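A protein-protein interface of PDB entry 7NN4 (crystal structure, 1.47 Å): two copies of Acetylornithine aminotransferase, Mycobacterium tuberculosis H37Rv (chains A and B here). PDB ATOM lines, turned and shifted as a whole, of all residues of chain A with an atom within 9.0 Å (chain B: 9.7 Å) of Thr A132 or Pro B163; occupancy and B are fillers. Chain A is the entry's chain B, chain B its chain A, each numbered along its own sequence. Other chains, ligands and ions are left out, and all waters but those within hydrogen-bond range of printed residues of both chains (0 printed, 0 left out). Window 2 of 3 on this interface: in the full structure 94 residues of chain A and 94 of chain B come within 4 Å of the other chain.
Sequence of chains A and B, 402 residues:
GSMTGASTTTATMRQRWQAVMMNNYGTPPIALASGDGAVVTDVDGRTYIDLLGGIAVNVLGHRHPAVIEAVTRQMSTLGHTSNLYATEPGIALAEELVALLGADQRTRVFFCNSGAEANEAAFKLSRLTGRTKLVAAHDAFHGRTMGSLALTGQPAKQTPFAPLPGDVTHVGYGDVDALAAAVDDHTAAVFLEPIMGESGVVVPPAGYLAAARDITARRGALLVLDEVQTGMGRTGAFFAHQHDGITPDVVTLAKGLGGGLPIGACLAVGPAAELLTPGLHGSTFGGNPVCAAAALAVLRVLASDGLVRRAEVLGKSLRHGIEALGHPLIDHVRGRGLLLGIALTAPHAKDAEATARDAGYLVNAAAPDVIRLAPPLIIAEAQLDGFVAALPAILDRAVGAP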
ATOM      1  N   PHE A 123      -9.225  18.393 -12.995  1.00  0.00           N
ATOM      2  CA  PHE A 123      -8.050  17.990 -13.769  1.00  0.00           C
ATOM      3  C   PHE A 123      -7.660  16.554 -13.422  1.00  0.00           C
ATOM      4  O   PHE A 123      -7.436  15.720 -14.309  1.00  0.00           O
ATOM      5  CB  PHE A 123      -6.908  18.972 -13.456  1.00  0.00           C
ATOM      6  CG  PHE A 123      -5.721  18.903 -14.402  1.00  0.00           C
ATOM      7  CD1 PHE A 123      -4.897  17.787 -14.427  1.00  0.00           C
ATOM      8  CD2 PHE A 123      -5.385  19.988 -15.189  1.00  0.00           C
ATOM      9  CE1 PHE A 123      -3.789  17.730 -15.269  1.00  0.00           C
ATOM     10  CE2 PHE A 123      -4.281  19.944 -16.038  1.00  0.00           C
ATOM     11  CZ  PHE A 123      -3.490  18.811 -16.081  1.00  0.00           C
ATOM     12  N   LYS A 124      -7.609  16.240 -12.128  1.00  0.00           N
ATOM     13  CA  LYS A 124      -7.233  14.891 -11.713  1.00  0.00           C
ATOM     14  C   LYS A 124      -8.277  13.869 -12.145  1.00  0.00           C
ATOM     15  O   LYS A 124      -7.923  12.777 -12.614  1.00  0.00           O
ATOM     16  CB  LYS A 124      -6.951  14.860 -10.209  1.00  0.00           C
ATOM     17  CG  LYS A 124      -5.690  15.650  -9.873  1.00  0.00           C
ATOM     18  CD  LYS A 124      -5.378  15.682  -8.374  1.00  0.00           C
ATOM     19  CE  LYS A 124      -4.951  14.307  -7.853  1.00  0.00           C
ATOM     20  NZ  LYS A 124      -4.509  14.372  -6.434  1.00  0.00           N
ATOM     21  N   SER A 126      -9.942  14.076 -14.851  1.00  0.00           N
ATOM     22  CA  SER A 126      -9.720  13.852 -16.277  1.00  0.00           C
ATOM     23  C   SER A 126      -8.581  12.871 -16.527  1.00  0.00           C
ATOM     24  O   SER A 126      -8.628  12.117 -17.505  1.00  0.00           O
ATOM     25  CB  SER A 126      -9.481  15.173 -17.019  1.00  0.00           C
ATOM     26  OG  SER A 126      -8.136  15.597 -16.902  1.00  0.00           O
ATOM     27  N   ARG A 127      -7.556  12.861 -15.663  1.00  0.00           N
ATOM     28  CA  ARG A 127      -6.467  11.899 -15.817  1.00  0.00           C
ATOM     29  C   ARG A 127      -6.963  10.466 -15.667  1.00  0.00           C
ATOM     30  O   ARG A 127      -6.452   9.559 -16.335  1.00  0.00           O
ATOM     31  CB  ARG A 127      -5.361  12.170 -14.792  1.00  0.00           C
ATOM     32  CG  ARG A 127      -4.525  13.406 -15.084  1.00  0.00           C
ATOM     33  CD  ARG A 127      -3.533  13.155 -16.212  1.00  0.00           C
ATOM     34  NE  ARG A 127      -2.452  14.140 -16.241  1.00  0.00           N
ATOM     35  CZ  ARG A 127      -2.353  15.127 -17.131  1.00  0.00           C
ATOM     36  NH1 ARG A 127      -3.283  15.291 -18.065  1.00  0.00           N
ATOM     37  NH2 ARG A 127      -1.319  15.965 -17.092  1.00  0.00           N
ATOM     38  N   LEU A 128      -7.950  10.237 -14.797  1.00  0.00           N
ATOM     39  CA  LEU A 128      -8.424   8.885 -14.535  1.00  0.00           C
ATOM     40  C   LEU A 128      -9.240   8.312 -15.689  1.00  0.00           C
ATOM     41  O   LEU A 128      -9.612   7.132 -15.638  1.00  0.00           O
ATOM     42  CB  LEU A 128      -9.223   8.863 -13.229  1.00  0.00           C
ATOM     43  CG  LEU A 128      -8.361   9.207 -12.013  1.00  0.00           C
ATOM     44  CD1 LEU A 128      -9.220   9.440 -10.770  1.00  0.00           C
ATOM     45  CD2 LEU A 128      -7.330   8.118 -11.751  1.00  0.00           C
ATOM     46  N   THR A 129      -9.535   9.112 -16.715  1.00  0.00           N
ATOM     47  CA  THR A 129     -10.133   8.581 -17.935  1.00  0.00           C
ATOM     48  C   THR A 129      -9.133   7.812 -18.789  1.00  0.00           C
ATOM     49  O   THR A 129      -9.540   7.200 -19.781  1.00  0.00           O
ATOM     50  CB  THR A 129     -10.692   9.713 -18.795  1.00  0.00           C
ATOM     51  OG1 THR A 129      -9.601  10.508 -19.266  1.00  0.00           O
ATOM     52  CG2 THR A 129     -11.667  10.593 -18.009  1.00  0.00           C
ATOM     53  N   GLY A 130      -7.844   7.842 -18.448  1.00  0.00           N
ATOM     54  CA  GLY A 130      -6.809   7.267 -19.284  1.00  0.00           C
ATOM     55  C   GLY A 130      -6.342   8.153 -20.418  1.00  0.00           C
ATOM     56  O   GLY A 130      -5.483   7.731 -21.204  1.00  0.00           O
ATOM     57  N   ARG A 131      -6.887   9.358 -20.541  1.00  0.00           N
ATOM     58  CA  ARG A 131      -6.501  10.302 -21.572  1.00  0.00           C
ATOM     59  C   ARG A 131      -5.788  11.476 -20.915  1.00  0.00           C
ATOM     60  O   ARG A 131      -6.056  11.820 -19.760  1.00  0.00           O
ATOM     61  CB  ARG A 131      -7.733  10.801 -22.335  1.00  0.00           C
ATOM     62  CG  ARG A 131      -8.592   9.687 -22.945  1.00  0.00           C
ATOM     63  CD  ARG A 131      -9.787  10.270 -23.688  1.00  0.00           C
ATOM     64  NE  ARG A 131     -10.626   9.244 -24.309  1.00  0.00           N
ATOM     65  CZ  ARG A 131     -11.652   9.507 -25.112  1.00  0.00           C
ATOM     66  NH1 ARG A 131     -11.968  10.763 -25.405  1.00  0.00           N
ATOM     67  NH2 ARG A 131     -12.357   8.508 -25.632  1.00  0.00           N
ATOM     68  N   THR A 132      -4.870  12.082 -21.655  1.00  0.00           N
ATOM     69  CA  THR A 132      -4.088  13.176 -21.114  1.00  0.00           C
ATOM     70  C   THR A 132      -4.277  14.491 -21.849  1.00  0.00           C
ATOM     71  O   THR A 132      -3.714  15.506 -21.425  1.00  0.00           O
ATOM     72  CB  THR A 132      -2.597  12.820 -21.114  1.00  0.00           C
ATOM     73  OG1 THR A 132      -2.203  12.463 -22.439  1.00  0.00           O
ATOM     74  CG2 THR A 132      -2.334  11.638 -20.194  1.00  0.00           C
ATOM     75  N   LYS A 133      -5.002  14.498 -22.962  1.00  0.00           N
ATOM     76  CA  LYS A 133      -5.220  15.746 -23.743  1.00  0.00           C
ATOM     77  C   LYS A 133      -6.416  16.535 -23.192  1.00  0.00           C
ATOM     78  O   LYS A 133      -7.409  15.955 -22.898  1.00  0.00           O
ATOM     79  CB  LYS A 133      -5.359  15.464 -25.241  1.00  0.00           C
ATOM     80  CG  LYS A 133      -4.045  15.235 -25.983  1.00  0.00           C
ATOM     81  CD  LYS A 133      -3.069  14.316 -25.284  1.00  0.00           C
ATOM     82  CE  LYS A 133      -1.703  14.279 -25.936  1.00  0.00           C
ATOM     83  NZ  LYS A 133      -0.765  13.375 -25.228  1.00  0.00           N
ATOM     84  N   LEU A 134      -6.246  17.841 -23.073  1.00  0.00           N
ATOM     85  CA  LEU A 134      -7.274  18.707 -22.532  1.00  0.00           C
ATOM     86  C   LEU A 134      -7.479  19.885 -23.466  1.00  0.00           C
ATOM     87  O   LEU A 134      -6.543  20.349 -24.120  1.00  0.00           O
ATOM     88  CB  LEU A 134      -6.825  19.228 -21.167  1.00  0.00           C
ATOM     89  CG  LEU A 134      -6.645  18.106 -20.141  1.00  0.00           C
ATOM     90  CD1 LEU A 134      -5.577  18.446 -19.119  1.00  0.00           C
ATOM     91  CD2 LEU A 134      -7.972  17.797 -19.464  1.00  0.00           C
ATOM     92  N   VAL A 135      -8.711  20.377 -23.506  1.00  0.00           N
ATOM     93  CA  VAL A 135      -9.069  21.523 -24.332  1.00  0.00           C
ATOM     94  C   VAL A 135      -9.720  22.585 -23.460  1.00  0.00           C
ATOM     95  O   VAL A 135     -10.584  22.276 -22.631  1.00  0.00           O
ATOM     96  CB  VAL A 135      -9.986  21.116 -25.499  1.00  0.00           C
ATOM     97  CG1 VAL A 135     -10.481  22.346 -26.263  1.00  0.00           C
ATOM     98  CG2 VAL A 135      -9.237  20.175 -26.408  1.00  0.00           C
ATOM     99  N   GLY A 147      -1.937  22.974 -12.136  1.00  0.00           N
ATOM    100  CA  GLY A 147      -2.859  22.304 -13.042  1.00  0.00           C
ATOM    101  C   GLY A 147      -3.906  23.246 -13.611  1.00  0.00           C
ATOM    102  O   GLY A 147      -4.149  23.282 -14.824  1.00  0.00           O
ATOM    103  N   LEU A 151      -4.882  25.103 -17.647  1.00  0.00           N
ATOM    104  CA  LEU A 151      -6.185  25.242 -18.294  1.00  0.00           C
ATOM    105  C   LEU A 151      -6.514  26.700 -18.585  1.00  0.00           C
ATOM    106  O   LEU A 151      -7.099  27.018 -19.631  1.00  0.00           O
ATOM    107  CB  LEU A 151      -7.256  24.639 -17.378  1.00  0.00           C
ATOM    108  CG  LEU A 151      -7.120  23.142 -17.138  1.00  0.00           C
ATOM    109  CD1 LEU A 151      -8.033  22.723 -15.987  1.00  0.00           C
ATOM    110  CD2 LEU A 151      -7.446  22.360 -18.406  1.00  0.00           C
ATOM    111  N   LEU A 164       4.149  23.978 -17.876  1.00  0.00           N
ATOM    112  CA  LEU A 164       2.921  23.614 -17.142  1.00  0.00           C
ATOM    113  C   LEU A 164       2.536  22.173 -17.492  1.00  0.00           C
ATOM    114  O   LEU A 164       2.897  21.712 -18.546  1.00  0.00           O
ATOM    115  CB  LEU A 164       1.796  24.584 -17.509  1.00  0.00           C
ATOM    116  CG  LEU A 164       2.087  26.064 -17.304  1.00  0.00           C
ATOM    117  CD1 LEU A 164       0.904  26.908 -17.753  1.00  0.00           C
ATOM    118  CD2 LEU A 164       2.380  26.365 -15.861  1.00  0.00           C
ATOM    119  N   PRO A 165       1.719  21.489 -16.676  1.00  0.00           N
ATOM    120  CA  PRO A 165       1.313  20.126 -16.962  1.00  0.00           C
ATOM    121  C   PRO A 165       0.480  20.087 -18.248  1.00  0.00           C
ATOM    122  O   PRO A 165      -0.248  20.962 -18.488  1.00  0.00           O
ATOM    123  CB  PRO A 165       0.517  19.671 -15.750  1.00  0.00           C
ATOM    124  CG  PRO A 165       0.067  20.948 -15.129  1.00  0.00           C
ATOM    125  CD  PRO A 165       1.141  21.968 -15.434  1.00  0.00           C
ATOM    126  N   GLY A 166       0.647  19.006 -18.998  1.00  0.00           N
ATOM    127  CA  GLY A 166       0.034  18.880 -20.326  1.00  0.00           C
ATOM    128  C   GLY A 166      -1.180  18.001 -20.332  1.00  0.00           C
ATOM    129  O   GLY A 166      -1.558  17.554 -19.294  1.00  0.00           O
ATOM    130  N   ASP A 167      -1.723  17.740 -21.509  1.00  0.00           N
ATOM    131  CA  ASP A 167      -1.368  18.397 -22.793  1.00  0.00           C
ATOM    132  C   ASP A 167      -2.573  19.250 -23.193  1.00  0.00           C
ATOM    133  O   ASP A 167      -3.570  18.697 -23.613  1.00  0.00           O
ATOM    134  CB  ASP A 167      -1.072  17.353 -23.868  1.00  0.00           C
ATOM    135  CG  ASP A 167       0.238  16.623 -23.640  1.00  0.00           C
ATOM    136  OD1 ASP A 167       1.184  17.248 -23.227  1.00  0.00           O
ATOM    137  OD2 ASP A 167       0.262  15.434 -23.861  1.00  0.00           O
ATOM    138  N   VAL A 168      -2.439  20.553 -23.070  1.00  0.00           N
ATOM    139  CA  VAL A 168      -3.620  21.435 -23.251  1.00  0.00           C
ATOM    140  C   VAL A 168      -3.599  22.151 -24.595  1.00  0.00           C
ATOM    141  O   VAL A 168      -2.586  22.671 -24.948  1.00  0.00           O
ATOM    142  CB  VAL A 168      -3.727  22.459 -22.107  1.00  0.00           C
ATOM    143  CG1 VAL A 168      -5.049  23.193 -22.173  1.00  0.00           C
ATOM    144  CG2 VAL A 168      -3.553  21.802 -20.754  1.00  0.00           C
ATOM    145  N   THR A 169      -4.733  22.130 -25.263  1.00  0.00           N
ATOM    146  CA  THR A 169      -4.928  22.877 -26.514  1.00  0.00           C
ATOM    147  C   THR A 169      -5.970  23.953 -26.223  1.00  0.00           C
ATOM    148  O   THR A 169      -6.968  23.624 -25.659  1.00  0.00           O
ATOM    149  CB  THR A 169      -5.446  21.976 -27.637  1.00  0.00           C
ATOM    150  OG1 THR A 169      -4.377  21.105 -27.966  1.00  0.00           O
ATOM    151  CG2 THR A 169      -5.831  22.765 -28.859  1.00  0.00           C
ATOM    152  N   ASP A 184     -11.014  15.038 -29.879  1.00  0.00           N
ATOM    153  CA  ASP A 184     -10.984  13.738 -30.539  1.00  0.00           C
ATOM    154  C   ASP A 184     -10.983  12.653 -29.464  1.00  0.00           C
ATOM    155  O   ASP A 184     -11.225  12.918 -28.283  1.00  0.00           O
ATOM    156  CB  ASP A 184      -9.825  13.654 -31.543  1.00  0.00           C
ATOM    157  CG  ASP A 184      -8.479  13.797 -30.882  1.00  0.00           C
ATOM    158  OD1 ASP A 184      -8.284  13.211 -29.792  1.00  0.00           O
ATOM    159  OD2 ASP A 184      -7.605  14.510 -31.419  1.00  0.00           O
ATOM    160  N   ASP A 185     -10.684  11.421 -29.872  1.00  0.00           N
ATOM    161  CA  ASP A 185     -10.741  10.284 -28.963  1.00  0.00           C
ATOM    162  C   ASP A 185      -9.572  10.224 -27.986  1.00  0.00           C
ATOM    163  O   ASP A 185      -9.521   9.304 -27.167  1.00  0.00           O
ATOM    164  CB  ASP A 185     -10.884   8.971 -29.744  1.00  0.00           C
ATOM    165  CG  ASP A 185      -9.660   8.647 -30.577  1.00  0.00           C
ATOM    166  OD1 ASP A 185      -9.075   9.582 -31.164  1.00  0.00           O
ATOM    167  OD2 ASP A 185      -9.291   7.456 -30.656  1.00  0.00           O
ATOM    168  N   HIS A 186      -8.641  11.174 -28.032  1.00  0.00           N
ATOM    169  CA  HIS A 186      -7.618  11.276 -27.002  1.00  0.00           C
ATOM    170  C   HIS A 186      -7.885  12.402 -26.019  1.00  0.00           C
ATOM    171  O   HIS A 186      -7.045  12.662 -25.152  1.00  0.00           O
ATOM    172  CB  HIS A 186      -6.232  11.429 -27.617  1.00  0.00           C
ATOM    173  CG  HIS A 186      -5.850  10.290 -28.507  1.00  0.00           C
ATOM    174  ND1 HIS A 186      -5.729  10.424 -29.872  1.00  0.00           N
ATOM    175  CD2 HIS A 186      -5.596   8.990 -28.230  1.00  0.00           C
ATOM    176  CE1 HIS A 186      -5.393   9.260 -30.397  1.00  0.00           C
ATOM    177  NE2 HIS A 186      -5.310   8.371 -29.424  1.00  0.00           N
ATOM    178  N   THR A 187      -9.031  13.066 -26.129  1.00  0.00           N
ATOM    179  CA  THR A 187      -9.333  14.229 -25.307  1.00  0.00           C
ATOM    180  C   THR A 187      -9.976  13.770 -24.002  1.00  0.00           C
ATOM    181  O   THR A 187     -11.072  13.199 -24.010  1.00  0.00           O
ATOM    182  CB  THR A 187     -10.268  15.166 -26.062  1.00  0.00           C
ATOM    183  OG1 THR A 187      -9.623  15.602 -27.265  1.00  0.00           O
ATOM    184  CG2 THR A 187     -10.572  16.391 -25.216  1.00  0.00           C
ATOM    185  N   ALA A 188      -9.285  14.013 -22.888  1.00  0.00           N
ATOM    186  CA  ALA A 188      -9.826  13.659 -21.581  1.00  0.00           C
ATOM    187  C   ALA A 188     -11.021  14.530 -21.222  1.00  0.00           C
ATOM    188  O   ALA A 188     -12.027  14.032 -20.702  1.00  0.00           O
ATOM    189  CB  ALA A 188      -8.738  13.812 -20.519  1.00  0.00           C
ATOM    190  N   ALA A 189     -10.929  15.830 -21.489  1.00  0.00           N
ATOM    191  CA  ALA A 189     -11.953  16.755 -21.025  1.00  0.00           C
ATOM    192  C   ALA A 189     -11.823  18.080 -21.750  1.00  0.00           C
ATOM    193  O   ALA A 189     -10.741  18.460 -22.201  1.00  0.00           O
ATOM    194  CB  ALA A 189     -11.836  16.999 -19.512  1.00  0.00           C
ATOM    195  N   THR B 145      -2.769  18.943  -5.098  1.00  0.00           N
ATOM    196  CA  THR B 145      -2.943  19.618  -6.374  1.00  0.00           C
ATOM    197  C   THR B 145      -1.770  19.250  -7.287  1.00  0.00           C
ATOM    198  O   THR B 145      -0.763  18.708  -6.836  1.00  0.00           O
ATOM    199  CB  THR B 145      -3.041  21.128  -6.155  1.00  0.00           C
ATOM    200  OG1 THR B 145      -1.920  21.564  -5.374  1.00  0.00           O
ATOM    201  CG2 THR B 145      -4.338  21.483  -5.408  1.00  0.00           C
ATOM    202  N   MET B 146      -1.906  19.530  -8.587  1.00  0.00           N
ATOM    203  CA  MET B 146      -0.969  18.945  -9.552  1.00  0.00           C
ATOM    204  C   MET B 146       0.479  19.347  -9.280  1.00  0.00           C
ATOM    205  O   MET B 146       1.384  18.509  -9.370  1.00  0.00           O
ATOM    206  CB  MET B 146      -1.384  19.285 -10.984  1.00  0.00           C
ATOM    207  CG  MET B 146      -2.635  18.541 -11.463  1.00  0.00           C
ATOM    208  SD  MET B 146      -2.435  16.740 -11.564  1.00  0.00           S
ATOM    209  CE  MET B 146      -1.298  16.653 -12.954  1.00  0.00           C
ATOM    210  N   GLY B 147       0.727  20.615  -8.948  1.00  0.00           N
ATOM    211  CA  GLY B 147       2.093  21.028  -8.660  1.00  0.00           C
ATOM    212  C   GLY B 147       2.598  20.449  -7.351  1.00  0.00           C
ATOM    213  O   GLY B 147       3.698  19.882  -7.276  1.00  0.00           O
ATOM    214  N   LEU B 149       1.469  17.839  -5.835  1.00  0.00           N
ATOM    215  CA  LEU B 149       1.545  16.384  -5.938  1.00  0.00           C
ATOM    216  C   LEU B 149       2.834  15.936  -6.623  1.00  0.00           C
ATOM    217  O   LEU B 149       3.346  14.852  -6.324  1.00  0.00           O
ATOM    218  CB  LEU B 149       0.334  15.860  -6.703  1.00  0.00           C
ATOM    219  CG  LEU B 149       0.219  14.352  -6.911  1.00  0.00           C
ATOM    220  CD1 LEU B 149       0.125  13.630  -5.563  1.00  0.00           C
ATOM    221  CD2 LEU B 149      -0.991  14.057  -7.784  1.00  0.00           C
ATOM    222  N   ALA B 150       3.368  16.750  -7.537  1.00  0.00           N
ATOM    223  CA  ALA B 150       4.660  16.430  -8.138  1.00  0.00           C
ATOM    224  C   ALA B 150       5.771  16.478  -7.100  1.00  0.00           C
ATOM    225  O   ALA B 150       6.757  15.734  -7.206  1.00  0.00           O
ATOM    226  CB  ALA B 150       4.963  17.397  -9.287  1.00  0.00           C
ATOM    227  N   GLN B 158       0.792   9.394  -7.187  1.00  0.00           N
ATOM    228  CA  GLN B 158       1.177  10.284  -8.303  1.00  0.00           C
ATOM    229  C   GLN B 158       0.914   9.621  -9.654  1.00  0.00           C
ATOM    230  O   GLN B 158       0.389  10.269 -10.516  1.00  0.00           O
ATOM    231  CB  GLN B 158       2.679  10.587  -8.269  1.00  0.00           C
ATOM    232  CG  GLN B 158       3.142  11.386  -7.067  1.00  0.00           C
ATOM    233  CD  GLN B 158       4.641  11.533  -7.051  1.00  0.00           C
ATOM    234  OE1 GLN B 158       5.368  10.567  -6.931  1.00  0.00           O
ATOM    235  NE2 GLN B 158       5.116  12.746  -7.169  1.00  0.00           N
ATOM    236  N   THR B 159       1.272   8.344  -9.765  1.00  0.00           N
ATOM    237  CA  THR B 159       1.181   7.591 -11.041  1.00  0.00           C
ATOM    238  C   THR B 159      -0.155   7.731 -11.767  1.00  0.00           C
ATOM    239  O   THR B 159      -0.125   7.988 -12.949  1.00  0.00           O
ATOM    240  CB  THR B 159       1.496   6.108 -10.862  1.00  0.00           C
ATOM    241  OG1 THR B 159       2.866   6.123 -10.483  1.00  0.00           O
ATOM    242  CG2 THR B 159       1.340   5.365 -12.168  1.00  0.00           C
ATOM    243  N   PRO B 160      -1.332   7.624 -11.118  1.00  0.00           N
ATOM    244  CA  PRO B 160      -2.601   7.773 -11.833  1.00  0.00           C
ATOM    245  C   PRO B 160      -2.856   9.116 -12.538  1.00  0.00           C
ATOM    246  O   PRO B 160      -3.610   9.148 -13.411  1.00  0.00           O
ATOM    247  CB  PRO B 160      -3.660   7.542 -10.758  1.00  0.00           C
ATOM    248  CG  PRO B 160      -2.942   6.749  -9.708  1.00  0.00           C
ATOM    249  CD  PRO B 160      -1.531   7.277  -9.731  1.00  0.00           C
ATOM    250  N   PHE B 161      -2.097  10.127 -12.141  1.00  0.00           N
ATOM    251  CA  PHE B 161      -2.305  11.506 -12.620  1.00  0.00           C
ATOM    252  C   PHE B 161      -1.163  11.975 -13.507  1.00  0.00           C
ATOM    253  O   PHE B 161      -1.167  13.087 -13.874  1.00  0.00           O
ATOM    254  CB  PHE B 161      -2.523  12.391 -11.389  1.00  0.00           C
ATOM    255  CG  PHE B 161      -3.600  11.853 -10.499  1.00  0.00           C
ATOM    256  CD1 PHE B 161      -4.923  11.942 -10.889  1.00  0.00           C
ATOM    257  CD2 PHE B 161      -3.301  11.247  -9.299  1.00  0.00           C
ATOM    258  CE1 PHE B 161      -5.928  11.405 -10.111  1.00  0.00           C
ATOM    259  CE2 PHE B 161      -4.313  10.738  -8.512  1.00  0.00           C
ATOM    260  CZ  PHE B 161      -5.618  10.819  -8.917  1.00  0.00           C
ATOM    261  N   ALA B 162      -0.234  11.086 -13.825  1.00  0.00           N
ATOM    262  CA  ALA B 162       0.891  11.466 -14.695  1.00  0.00           C
ATOM    263  C   ALA B 162       0.399  11.808 -16.101  1.00  0.00           C
ATOM    264  O   ALA B 162      -0.528  11.188 -16.553  1.00  0.00           O
ATOM    265  CB  ALA B 162       1.917  10.367 -14.723  1.00  0.00           C
ATOM    266  N   PRO B 163       1.008  12.773 -16.812  1.00  0.00           N
ATOM    267  CA  PRO B 163       2.185  13.469 -16.341  1.00  0.00           C
ATOM    268  C   PRO B 163       1.950  14.614 -15.348  1.00  0.00           C
ATOM    269  O   PRO B 163       1.041  15.316 -15.467  1.00  0.00           O
ATOM    270  CB  PRO B 163       2.806  14.041 -17.611  1.00  0.00           C
ATOM    271  CG  PRO B 163       1.664  14.224 -18.547  1.00  0.00           C
ATOM    272  CD  PRO B 163       0.634  13.195 -18.144  1.00  0.00           C
ATOM    273  N   LEU B 164       2.864  14.725 -14.402  1.00  0.00           N
ATOM    274  CA  LEU B 164       2.777  15.819 -13.413  1.00  0.00           C
ATOM    275  C   LEU B 164       3.747  16.917 -13.833  1.00  0.00           C
ATOM    276  O   LEU B 164       4.664  16.663 -14.573  1.00  0.00           O
ATOM    277  CB  LEU B 164       3.152  15.282 -12.029  1.00  0.00           C
ATOM    278  CG  LEU B 164       2.317  14.119 -11.508  1.00  0.00           C
ATOM    279  CD1 LEU B 164       2.797  13.688 -10.143  1.00  0.00           C
ATOM    280  CD2 LEU B 164       0.857  14.485 -11.433  1.00  0.00           C
ATOM    281  N   PRO B 165       3.596  18.127 -13.288  1.00  0.00           N
ATOM    282  CA  PRO B 165       4.525  19.210 -13.546  1.00  0.00           C
ATOM    283  C   PRO B 165       5.964  18.770 -13.183  1.00  0.00           C
ATOM    284  O   PRO B 165       6.164  18.179 -12.187  1.00  0.00           O
ATOM    285  CB  PRO B 165       4.058  20.263 -12.529  1.00  0.00           C
ATOM    286  CG  PRO B 165       2.621  19.991 -12.322  1.00  0.00           C
ATOM    287  CD  PRO B 165       2.500  18.489 -12.399  1.00  0.00           C
ATOM    288  N   GLY B 166       6.937  19.117 -14.025  1.00  0.00           N
ATOM    289  CA  GLY B 166       8.335  18.703 -13.800  1.00  0.00           C
ATOM    290  C   GLY B 166       9.201  19.846 -13.329  1.00  0.00           C
ATOM    291  O   GLY B 166       8.698  20.922 -13.162  1.00  0.00           O
ATOM    292  N   ASP B 167      10.498  19.618 -13.159  1.00  0.00           N
ATOM    293  CA  ASP B 167      11.190  18.316 -13.309  1.00  0.00           C
ATOM    294  C   ASP B 167      11.663  17.942 -11.913  1.00  0.00           C
ATOM    295  O   ASP B 167      12.569  18.544 -11.430  1.00  0.00           O
ATOM    296  CB  ASP B 167      12.368  18.466 -14.263  1.00  0.00           C
ATOM    297  CG  ASP B 167      11.943  18.642 -15.708  1.00  0.00           C
ATOM    298  OD1 ASP B 167      10.841  18.230 -16.046  1.00  0.00           O
ATOM    299  OD2 ASP B 167      12.750  19.157 -16.482  1.00  0.00           O
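The guanidinium group (NH1) of Arg A127 sits at hydrogen-bond distance from the backbone carbonyl oxygen (O) of Thr A132, at 3.4 Å.
The backbone carbonyl oxygen of Thr A132 sits at hydrogen-bond distance from the backbone NH of Asp A167 (3.0 Å).
The side-chain hydroxyl (OG1) of Thr A132 sits at hydrogen-bond distance from the side-chain amino group (NZ) of Lys A133.
NE2 of Gln B158 sits at hydrogen-bond distance from O of Leu B149, at 2.9 Å.
The backbone carbonyl oxygen (O) of Phe A123 is in hydrogen-bond range of the side-chain hydroxyl (OG) of Ser A126, at 2.7 Å.
NH2 of Arg A127 is in hydrogen-bond range of O of Gly A166.
Among the printed residues, pairs that only touch across the chains: Phe A123 with Met B146 (3.6 Å), Lys A124 with Met B146 (3.8 Å), Lys A124 with Leu B149 (3.8 Å), Lys A124 with Phe B161 (3.5 Å), Arg A127 with Pro B160 (3.8 Å), Arg A127 with Ala B162 (3.5 Å), Leu A128 with Pro B160 (3.8 Å), Leu A128 with Phe B161 (3.8 Å), Thr A132 with Pro B163 (3.9 Å), Gly A147 with Met B146 (3.9 Å) and Pro A165 with Pro B165 (3.9 Å).
The backbone carbonyl oxygen (O) of Phe B161 is in hydrogen-bond range of the guanidinium group (NE) of Arg A127 (2.9 Å).
The backbone carbonyl oxygen of Pro B163 is in hydrogen-bond range of the guanidinium group of Arg A127, at 2.9 Å.
Pro A165 touches its own counterpart, Pro B165.
5 positions are printed for both chains.
Of the 13 pairs that touch across the chains among the printed residues, 1 has its exchanged pair printed and touching as well.
Printed residues of chain B within 4 Å of Phe A123: Met B146 (3.6 Å).
Thr A132 touches one residue of chain B.
No residue of chain B comes within 4 Å of Lys A133.
No residue of chain B comes within 4 Å of Gly A166.
Thr A187 touches none of the printed residues of chain B.
Of the printed residues of chain A, Leu B149 touches Lys A124 (3.8 Å).
Printed residues of chain A within 4 Å of Pro B160: Arg A127 and Leu A128.
Printed residues of chain A within 4 Å of Phe B161: Lys A124, Arg A127 and Leu A128.
Ala B162 touches just one residue of chain A: Arg A127 (3.5 Å).
Pro B163 touches just these residues of chain A: Arg A127 and Thr A132.
Of the printed residues of chain A, Pro B165 touches Pro A165 (3.9 Å).
The nearest residue of chain B that does not touch Thr A132 is Ala B162 (4.1 Å).
Along chain B the printed residues that touch a printed residue of chain A span positions 146 to 165.
Of the 26 printed residues of chain A, 7 touch a printed residue of chain B.
Printed residues of chain A that touch a printed residue of chain B: Phe A123, Lys A124, Arg A127, Leu A128, Thr A132, Gly A147 and Pro A165.
Among the printed residues, 13 pairs touch across the chains.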
